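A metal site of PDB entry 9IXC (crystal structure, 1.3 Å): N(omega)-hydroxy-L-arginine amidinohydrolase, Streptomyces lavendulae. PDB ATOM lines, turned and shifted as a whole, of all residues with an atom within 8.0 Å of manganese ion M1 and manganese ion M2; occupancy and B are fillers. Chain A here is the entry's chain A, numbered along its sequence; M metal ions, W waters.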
ATOM      1  N   MET A  18      31.349   4.087  21.764  1.00  0.00           N
ATOM      2  CA  MET A  18      30.162   4.595  22.443  1.00  0.00           C
ATOM      3  C   MET A  18      29.702   3.696  23.589  1.00  0.00           C
ATOM      4  O   MET A  18      29.139   4.195  24.570  1.00  0.00           O
ATOM      5  CB  MET A  18      29.040   4.903  21.447  1.00  0.00           C
ATOM      6  CG  MET A  18      29.343   6.169  20.668  1.00  0.00           C
ATOM      7  SD  MET A  18      28.024   6.541  19.511  1.00  0.00           S
ATOM      8  CE  MET A  18      28.718   7.917  18.645  1.00  0.00           C
ATOM      9  N   THR A  85      23.948   4.523  22.245  1.00  0.00           N
ATOM     10  CA  THR A  85      23.473   5.187  21.033  1.00  0.00           C
ATOM     11  C   THR A  85      22.072   5.741  21.254  1.00  0.00           C
ATOM     12  O   THR A  85      21.328   5.309  22.138  1.00  0.00           O
ATOM     13  CB  THR A  85      23.418   4.240  19.832  1.00  0.00           C
ATOM     14  OG1 THR A  85      22.501   3.166  20.103  1.00  0.00           O
ATOM     15  CG2 THR A  85      24.810   3.675  19.477  1.00  0.00           C
ATOM     16  N   CYS A  86      21.719   6.729  20.426  1.00  0.00           N
ATOM     17  CA  CYS A  86      20.356   7.249  20.456  1.00  0.00           C
ATOM     18  C   CYS A  86      19.329   6.155  20.194  1.00  0.00           C
ATOM     19  O   CYS A  86      18.184   6.265  20.642  1.00  0.00           O
ATOM     20  CB  CYS A  86      20.185   8.379  19.442  1.00  0.00           C
ATOM     21  SG  CYS A  86      21.004   9.909  19.880  1.00  0.00           S
ATOM     22  N   SER A  87      19.705   5.111  19.456  1.00  0.00           N
ATOM     23  CA  SER A  87      18.769   4.052  19.082  1.00  0.00           C
ATOM     24  C   SER A  87      18.192   3.303  20.269  1.00  0.00           C
ATOM     25  O   SER A  87      17.122   2.703  20.128  1.00  0.00           O
ATOM     26  CB  SER A  87      19.477   3.065  18.149  1.00  0.00           C
ATOM     27  OG  SER A  87      19.706   3.673  16.901  1.00  0.00           O
ATOM     28  N   TYR A 107      14.567  16.631  22.390  1.00  0.00           N
ATOM     29  CA  TYR A 107      15.498  15.734  21.707  1.00  0.00           C
ATOM     30  C   TYR A 107      16.671  16.614  21.261  1.00  0.00           C
ATOM     31  O   TYR A 107      16.595  17.317  20.247  1.00  0.00           O
ATOM     32  CB  TYR A 107      14.792  15.023  20.568  1.00  0.00           C
ATOM     33  CG  TYR A 107      15.502  13.787  20.052  1.00  0.00           C
ATOM     34  CD1 TYR A 107      16.570  13.900  19.172  1.00  0.00           C
ATOM     35  CD2 TYR A 107      15.092  12.506  20.433  1.00  0.00           C
ATOM     36  CE1 TYR A 107      17.217  12.766  18.693  1.00  0.00           C
ATOM     37  CE2 TYR A 107      15.735  11.378  19.961  1.00  0.00           C
ATOM     38  CZ  TYR A 107      16.787  11.495  19.083  1.00  0.00           C
ATOM     39  OH  TYR A 107      17.426  10.354  18.606  1.00  0.00           O
ATOM     40  N   ILE A 108      17.726  16.610  22.054  1.00  0.00           N
ATOM     41  CA  ILE A 108      18.833  17.549  21.929  1.00  0.00           C
ATOM     42  C   ILE A 108      19.916  16.831  21.127  1.00  0.00           C
ATOM     43  O   ILE A 108      20.520  15.875  21.617  1.00  0.00           O
ATOM     44  CB  ILE A 108      19.329  18.020  23.296  1.00  0.00           C
ATOM     45  CG1 ILE A 108      18.146  18.494  24.157  1.00  0.00           C
ATOM     46  CG2 ILE A 108      20.388  19.104  23.151  1.00  0.00           C
ATOM     47  CD1 ILE A 108      18.549  19.026  25.511  1.00  0.00           C
ATOM     48  N   ASP A 109      20.156  17.274  19.899  1.00  0.00           N
ATOM     49  CA  ASP A 109      20.941  16.507  18.956  1.00  0.00           C
ATOM     50  C   ASP A 109      21.362  17.445  17.842  1.00  0.00           C
ATOM     51  O   ASP A 109      20.583  18.298  17.425  1.00  0.00           O
ATOM     52  CB  ASP A 109      20.031  15.386  18.411  1.00  0.00           C
ATOM     53  CG  ASP A 109      20.795  14.238  17.763  1.00  0.00           C
ATOM     54  OD1 ASP A 109      21.753  14.530  17.000  1.00  0.00           O
ATOM     55  OD2 ASP A 109      20.427  13.062  18.020  1.00  0.00           O
ATOM     56  N   GLY A 110      22.587  17.274  17.343  1.00  0.00           N
ATOM     57  CA  GLY A 110      22.989  18.025  16.155  1.00  0.00           C
ATOM     58  C   GLY A 110      22.246  17.610  14.902  1.00  0.00           C
ATOM     59  O   GLY A 110      22.210  18.372  13.927  1.00  0.00           O
ATOM     60  N   HIS A 111      21.651  16.413  14.917  1.00  0.00           N
ATOM     61  CA  HIS A 111      20.859  15.848  13.822  1.00  0.00           C
ATOM     62  C   HIS A 111      19.389  15.830  14.183  1.00  0.00           C
ATOM     63  O   HIS A 111      18.997  16.003  15.338  1.00  0.00           O
ATOM     64  CB  HIS A 111      21.293  14.398  13.563  1.00  0.00           C
ATOM     65  CG  HIS A 111      22.740  14.247  13.235  1.00  0.00           C
ATOM     66  ND1 HIS A 111      23.703  14.003  14.187  1.00  0.00           N
ATOM     67  CD2 HIS A 111      23.384  14.287  12.049  1.00  0.00           C
ATOM     68  CE1 HIS A 111      24.890  13.915  13.600  1.00  0.00           C
ATOM     69  NE2 HIS A 111      24.709  14.064  12.293  1.00  0.00           N
ATOM     70  N   GLY A 112      18.547  15.581  13.162  1.00  0.00           N
ATOM     71  CA  GLY A 112      17.125  15.396  13.408  1.00  0.00           C
ATOM     72  C   GLY A 112      16.711  14.000  13.813  1.00  0.00           C
ATOM     73  O   GLY A 112      15.657  13.829  14.430  1.00  0.00           O
ATOM     74  N   ASP A 113      17.516  12.982  13.464  1.00  0.00           N
ATOM     75  CA  ASP A 113      17.203  11.574  13.746  1.00  0.00           C
ATOM     76  C   ASP A 113      15.756  11.234  13.334  1.00  0.00           C
ATOM     77  O   ASP A 113      15.040  10.494  14.018  1.00  0.00           O
ATOM     78  CB  ASP A 113      17.486  11.190  15.201  1.00  0.00           C
ATOM     79  CG  ASP A 113      18.962  11.190  15.538  1.00  0.00           C
ATOM     80  OD1 ASP A 113      19.791  11.544  14.676  1.00  0.00           O
ATOM     81  OD2 ASP A 113      19.286  10.826  16.675  1.00  0.00           O
ATOM     82  N   TYR A 124      21.237   3.947   8.584  1.00  0.00           N
ATOM     83  CA  TYR A 124      21.643   3.907   9.989  1.00  0.00           C
ATOM     84  C   TYR A 124      20.432   4.052  10.905  1.00  0.00           C
ATOM     85  O   TYR A 124      19.706   5.052  10.847  1.00  0.00           O
ATOM     86  CB  TYR A 124      22.682   4.984  10.244  1.00  0.00           C
ATOM     87  CG  TYR A 124      23.162   5.033  11.664  1.00  0.00           C
ATOM     88  CD1 TYR A 124      23.454   3.861  12.368  1.00  0.00           C
ATOM     89  CD2 TYR A 124      23.326   6.246  12.307  1.00  0.00           C
ATOM     90  CE1 TYR A 124      23.900   3.905  13.679  1.00  0.00           C
ATOM     91  CE2 TYR A 124      23.759   6.306  13.627  1.00  0.00           C
ATOM     92  CZ  TYR A 124      24.043   5.138  14.310  1.00  0.00           C
ATOM     93  OH  TYR A 124      24.467   5.191  15.617  1.00  0.00           O
ATOM     94  N   LEU A 125      20.222   3.044  11.761  1.00  0.00           N
ATOM     95  CA  LEU A 125      19.129   3.064  12.726  1.00  0.00           C
ATOM     96  C   LEU A 125      19.166   4.317  13.595  1.00  0.00           C
ATOM     97  O   LEU A 125      18.114   4.870  13.939  1.00  0.00           O
ATOM     98  CB  LEU A 125      19.195   1.797  13.597  1.00  0.00           C
ATOM     99  CG  LEU A 125      18.009   1.575  14.541  1.00  0.00           C
ATOM    100  CD1 LEU A 125      16.731   1.309  13.757  1.00  0.00           C
ATOM    101  CD2 LEU A 125      18.305   0.414  15.473  1.00  0.00           C
ATOM    102  N   GLY A 126      20.356   4.776  13.966  1.00  0.00           N
ATOM    103  CA  GLY A 126      20.481   5.948  14.806  1.00  0.00           C
ATOM    104  C   GLY A 126      19.900   7.206  14.199  1.00  0.00           C
ATOM    105  O   GLY A 126      19.529   8.134  14.940  1.00  0.00           O
ATOM    106  N   GLY A 127      19.789   7.267  12.875  1.00  0.00           N
ATOM    107  CA  GLY A 127      19.162   8.388  12.208  1.00  0.00           C
ATOM    108  C   GLY A 127      17.657   8.271  12.066  1.00  0.00           C
ATOM    109  O   GLY A 127      17.055   9.127  11.398  1.00  0.00           O
ATOM    110  N   MET A 128      17.048   7.256  12.671  1.00  0.00           N
ATOM    111  CA  MET A 128      15.629   6.926  12.527  1.00  0.00           C
ATOM    112  C   MET A 128      14.901   6.883  13.856  1.00  0.00           C
ATOM    113  O   MET A 128      13.776   6.364  13.939  1.00  0.00           O
ATOM    114  CB  MET A 128      15.483   5.575  11.799  1.00  0.00           C
ATOM    115  CG  MET A 128      16.246   5.499  10.475  1.00  0.00           C
ATOM    116  SD  MET A 128      16.565   3.813   9.846  1.00  0.00           S
ATOM    117  CE  MET A 128      14.902   3.243   9.496  1.00  0.00           C
ATOM    118  N   VAL A 129      15.496   7.422  14.920  1.00  0.00           N
ATOM    119  CA  VAL A 129      14.999   7.193  16.279  1.00  0.00           C
ATOM    120  C   VAL A 129      13.739   8.008  16.569  1.00  0.00           C
ATOM    121  O   VAL A 129      12.735   7.471  17.044  1.00  0.00           O
ATOM    122  CB  VAL A 129      16.109   7.501  17.295  1.00  0.00           C
ATOM    123  CG1 VAL A 129      15.575   7.395  18.713  1.00  0.00           C
ATOM    124  CG2 VAL A 129      17.313   6.581  17.066  1.00  0.00           C
ATOM    125  N   LEU A 130      13.800   9.315  16.321  1.00  0.00           N
ATOM    126  CA  LEU A 130      12.677  10.156  16.723  1.00  0.00           C
ATOM    127  C   LEU A 130      11.471   9.900  15.826  1.00  0.00           C
ATOM    128  O   LEU A 130      10.334   9.915  16.303  1.00  0.00           O
ATOM    129  CB  LEU A 130      13.096  11.630  16.727  1.00  0.00           C
ATOM    130  CG  LEU A 130      12.032  12.637  17.184  1.00  0.00           C
ATOM    131  CD1 LEU A 130      11.555  12.321  18.597  1.00  0.00           C
ATOM    132  CD2 LEU A 130      12.606  14.042  17.096  1.00  0.00           C
ATOM    133  N   LEU A 152      13.064  19.219  18.637  1.00  0.00           N
ATOM    134  CA  LEU A 152      14.478  19.086  18.348  1.00  0.00           C
ATOM    135  C   LEU A 152      15.204  20.342  18.818  1.00  0.00           C
ATOM    136  O   LEU A 152      14.787  21.466  18.484  1.00  0.00           O
ATOM    137  CB  LEU A 152      14.671  18.865  16.848  1.00  0.00           C
ATOM    138  CG  LEU A 152      14.358  17.437  16.385  1.00  0.00           C
ATOM    139  CD1 LEU A 152      14.184  17.380  14.879  1.00  0.00           C
ATOM    140  CD2 LEU A 152      15.475  16.477  16.828  1.00  0.00           C
ATOM    141  N   SER A 155      19.563  21.088  16.617  1.00  0.00           N
ATOM    142  CA  SER A 155      19.728  20.466  15.315  1.00  0.00           C
ATOM    143  C   SER A 155      20.008  21.523  14.257  1.00  0.00           C
ATOM    144  O   SER A 155      19.503  22.657  14.317  1.00  0.00           O
ATOM    145  CB  SER A 155      18.462  19.693  14.962  1.00  0.00           C
ATOM    146  OG  SER A 155      18.043  18.887  16.050  1.00  0.00           O
ATOM    147  N   HIS A 196      16.429  14.039  26.121  1.00  0.00           N
ATOM    148  CA  HIS A 196      17.302  13.095  25.423  1.00  0.00           C
ATOM    149  C   HIS A 196      18.445  13.884  24.803  1.00  0.00           C
ATOM    150  O   HIS A 196      18.198  14.811  24.034  1.00  0.00           O
ATOM    151  CB  HIS A 196      16.481  12.406  24.323  1.00  0.00           C
ATOM    152  CG  HIS A 196      17.300  11.566  23.373  1.00  0.00           C
ATOM    153  ND1 HIS A 196      17.240  10.189  23.374  1.00  0.00           N
ATOM    154  CD2 HIS A 196      18.164  11.909  22.398  1.00  0.00           C
ATOM    155  CE1 HIS A 196      18.064   9.723  22.434  1.00  0.00           C
ATOM    156  NE2 HIS A 196      18.637  10.754  21.841  1.00  0.00           N
ATOM    157  N   ILE A 197      19.700  13.544  25.126  1.00  0.00           N
ATOM    158  CA  ILE A 197      20.847  14.269  24.575  1.00  0.00           C
ATOM    159  C   ILE A 197      21.761  13.335  23.805  1.00  0.00           C
ATOM    160  O   ILE A 197      22.183  12.289  24.325  1.00  0.00           O
ATOM    161  CB  ILE A 197      21.663  14.991  25.659  1.00  0.00           C
ATOM    162  CG1 ILE A 197      20.784  15.915  26.482  1.00  0.00           C
ATOM    163  CG2 ILE A 197      22.812  15.778  25.002  1.00  0.00           C
ATOM    164  CD1 ILE A 197      21.528  16.481  27.663  1.00  0.00           C
ATOM    165  N   ASP A 198      22.088  13.720  22.568  1.00  0.00           N
ATOM    166  CA  ASP A 198      23.186  13.162  21.779  1.00  0.00           C
ATOM    167  C   ASP A 198      24.302  14.184  21.825  1.00  0.00           C
ATOM    168  O   ASP A 198      24.132  15.334  21.391  1.00  0.00           O
ATOM    169  CB  ASP A 198      22.655  12.997  20.347  1.00  0.00           C
ATOM    170  CG  ASP A 198      23.698  12.533  19.328  1.00  0.00           C
ATOM    171  OD1 ASP A 198      24.903  12.624  19.572  1.00  0.00           O
ATOM    172  OD2 ASP A 198      23.241  12.110  18.246  1.00  0.00           O
ATOM    173  N   TRP A 199      25.470  13.780  22.340  1.00  0.00           N
ATOM    174  CA  TRP A 199      26.561  14.746  22.532  1.00  0.00           C
ATOM    175  C   TRP A 199      27.081  15.378  21.249  1.00  0.00           C
ATOM    176  O   TRP A 199      27.781  16.401  21.333  1.00  0.00           O
ATOM    177  CB  TRP A 199      27.713  14.149  23.355  1.00  0.00           C
ATOM    178  CG  TRP A 199      27.274  13.728  24.721  1.00  0.00           C
ATOM    179  CD1 TRP A 199      27.306  12.459  25.216  1.00  0.00           C
ATOM    180  CD2 TRP A 199      26.689  14.547  25.742  1.00  0.00           C
ATOM    181  NE1 TRP A 199      26.800  12.438  26.493  1.00  0.00           N
ATOM    182  CE2 TRP A 199      26.413  13.703  26.847  1.00  0.00           C
ATOM    183  CE3 TRP A 199      26.391  15.906  25.851  1.00  0.00           C
ATOM    184  CZ2 TRP A 199      25.840  14.174  28.026  1.00  0.00           C
ATOM    185  CZ3 TRP A 199      25.825  16.365  27.016  1.00  0.00           C
ATOM    186  CH2 TRP A 199      25.559  15.503  28.098  1.00  0.00           C
ATOM    187  N   ASP A 200      26.752  14.854  20.061  1.00  0.00           N
ATOM    188  CA  ASP A 200      27.171  15.546  18.847  1.00  0.00           C
ATOM    189  C   ASP A 200      26.463  16.881  18.657  1.00  0.00           C
ATOM    190  O   ASP A 200      26.786  17.609  17.728  1.00  0.00           O
ATOM    191  CB  ASP A 200      27.107  14.658  17.591  1.00  0.00           C
ATOM    192  CG  ASP A 200      25.692  14.272  17.149  1.00  0.00           C
ATOM    193  OD1 ASP A 200      24.708  14.984  17.447  1.00  0.00           O
ATOM    194  OD2 ASP A 200      25.598  13.210  16.496  1.00  0.00           O
ATOM    195  N   VAL A 201      25.517  17.222  19.534  1.00  0.00           N
ATOM    196  CA  VAL A 201      24.954  18.567  19.543  1.00  0.00           C
ATOM    197  C   VAL A 201      26.006  19.623  19.891  1.00  0.00           C
ATOM    198  O   VAL A 201      25.858  20.789  19.495  1.00  0.00           O
ATOM    199  CB  VAL A 201      23.724  18.658  20.466  1.00  0.00           C
ATOM    200  CG1 VAL A 201      24.151  18.660  21.943  1.00  0.00           C
ATOM    201  CG2 VAL A 201      22.876  19.893  20.113  1.00  0.00           C
ATOM    202  N   ALA A 240      23.447  10.104  25.630  1.00  0.00           N
ATOM    203  CA  ALA A 240      23.825   9.177  24.586  1.00  0.00           C
ATOM    204  C   ALA A 240      24.972   9.687  23.716  1.00  0.00           C
ATOM    205  O   ALA A 240      25.158  10.893  23.529  1.00  0.00           O
ATOM    206  CB  ALA A 240      22.616   8.857  23.674  1.00  0.00           C
ATOM    207  N   GLU A 241      25.740   8.730  23.202  1.00  0.00           N
ATOM    208  CA  GLU A 241      26.700   8.938  22.094  1.00  0.00           C
ATOM    209  C   GLU A 241      27.944   9.726  22.521  1.00  0.00           C
ATOM    210  O   GLU A 241      28.348  10.702  21.867  1.00  0.00           O
ATOM    211  CB  GLU A 241      26.034   9.518  20.849  1.00  0.00           C
ATOM    212  CG  GLU A 241      24.771   8.749  20.467  1.00  0.00           C
ATOM    213  CD  GLU A 241      24.622   8.436  18.994  1.00  0.00           C
ATOM    214  OE1 GLU A 241      25.429   8.935  18.166  1.00  0.00           O
ATOM    215  OE2 GLU A 241      23.663   7.715  18.659  1.00  0.00           O
HETATM  216 MN    MN M   1      21.263  11.102  17.698  1.00  0.00          MN
HETATM  217 MN    MN M   2      23.406  13.350  16.341  1.00  0.00          MN
HETATM  218  O   HOH W   1      22.085   9.217  16.905  1.00  0.00           O
HETATM  219  O   HOH W   2      22.144  11.657  15.637  1.00  0.00           O
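Manganese ion M2 is bound by OD1 of Asp 109 (2.1 Å).
The side-chain carboxylate (OD2) of Asp 200 is bound to manganese ion M2 (2.2 Å).
Water W2 is bound to manganese ion M2 (2.2 Å).
ND1 of His 111 is bound to manganese ion M2, 2.3 Å away.
Manganese ion M2 is bound by OD2 of Asp 198 (2.3 Å).
Manganese ion M2 is bound by OD1 of Asp 200.
Manganese ion M2 has six donor atoms within binding distance.
Of the 28 residues printed, 4 come within 4 Å of manganese ion M2.
The nearest printed residue that does not touch manganese ion M2 is Gly 110 (4.1 Å).
Four residues have an atom within 4 Å of manganese ion M1: Cys 86, Asp 109, Asp 113 and Asp 198.
Along chain A the residues within 4 Å of manganese ion M1 span positions 86 to 198.
The nearest printed residue that does not touch manganese ion M1 is Tyr 107 (4.01 Å).
Water W1 bridges the side-chain carboxylate of Glu 241 (2.8 Å) and the backbone carbonyl oxygen of Gly 126 (3.4 Å).
Manganese ion M1 is bound by OD2 of Asp 109.
Manganese ion M1 is bound by water W1 (2.2 Å).
OD2 of Asp 113 is bound to manganese ion M1 (2.2 Å).
OD2 of Asp 198 binds manganese ion M1, at 2.3 Å.
Manganese ion M1 is bound by water W2.
Manganese ion M1 is bound by SG of Cys 86 (2.5 Å).
The backbone carbonyl oxygen of Ile 108 sits at hydrogen-bond distance from the backbone NH of Asp 198 (2.8 Å).
N of Cys 86 is in hydrogen-bond range of OE2 of Glu 241 (2.8 Å).
The backbone carbonyl oxygen (O) of His 111 lies within hydrogen-bond range of the side-chain hydroxyl (OG) of Ser 155 (3.1 Å).
The backbone carbonyl oxygen of Asp 109 is in hydrogen-bond range of the side-chain hydroxyl of Ser 155 (2.9 Å).
SG of Cys 86 sits close to NE2 of His 196 (3.2 Å).
OD2 of Asp 113 lies close to OH of Tyr 107 (2.7 Å).
N of Gly 110 lies close to OD1 of Asp 200, at 3.1 Å.
The backbone NH (N) of Leu 130 sits at hydrogen-bond distance from the backbone carbonyl oxygen (O) of Asp 113.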
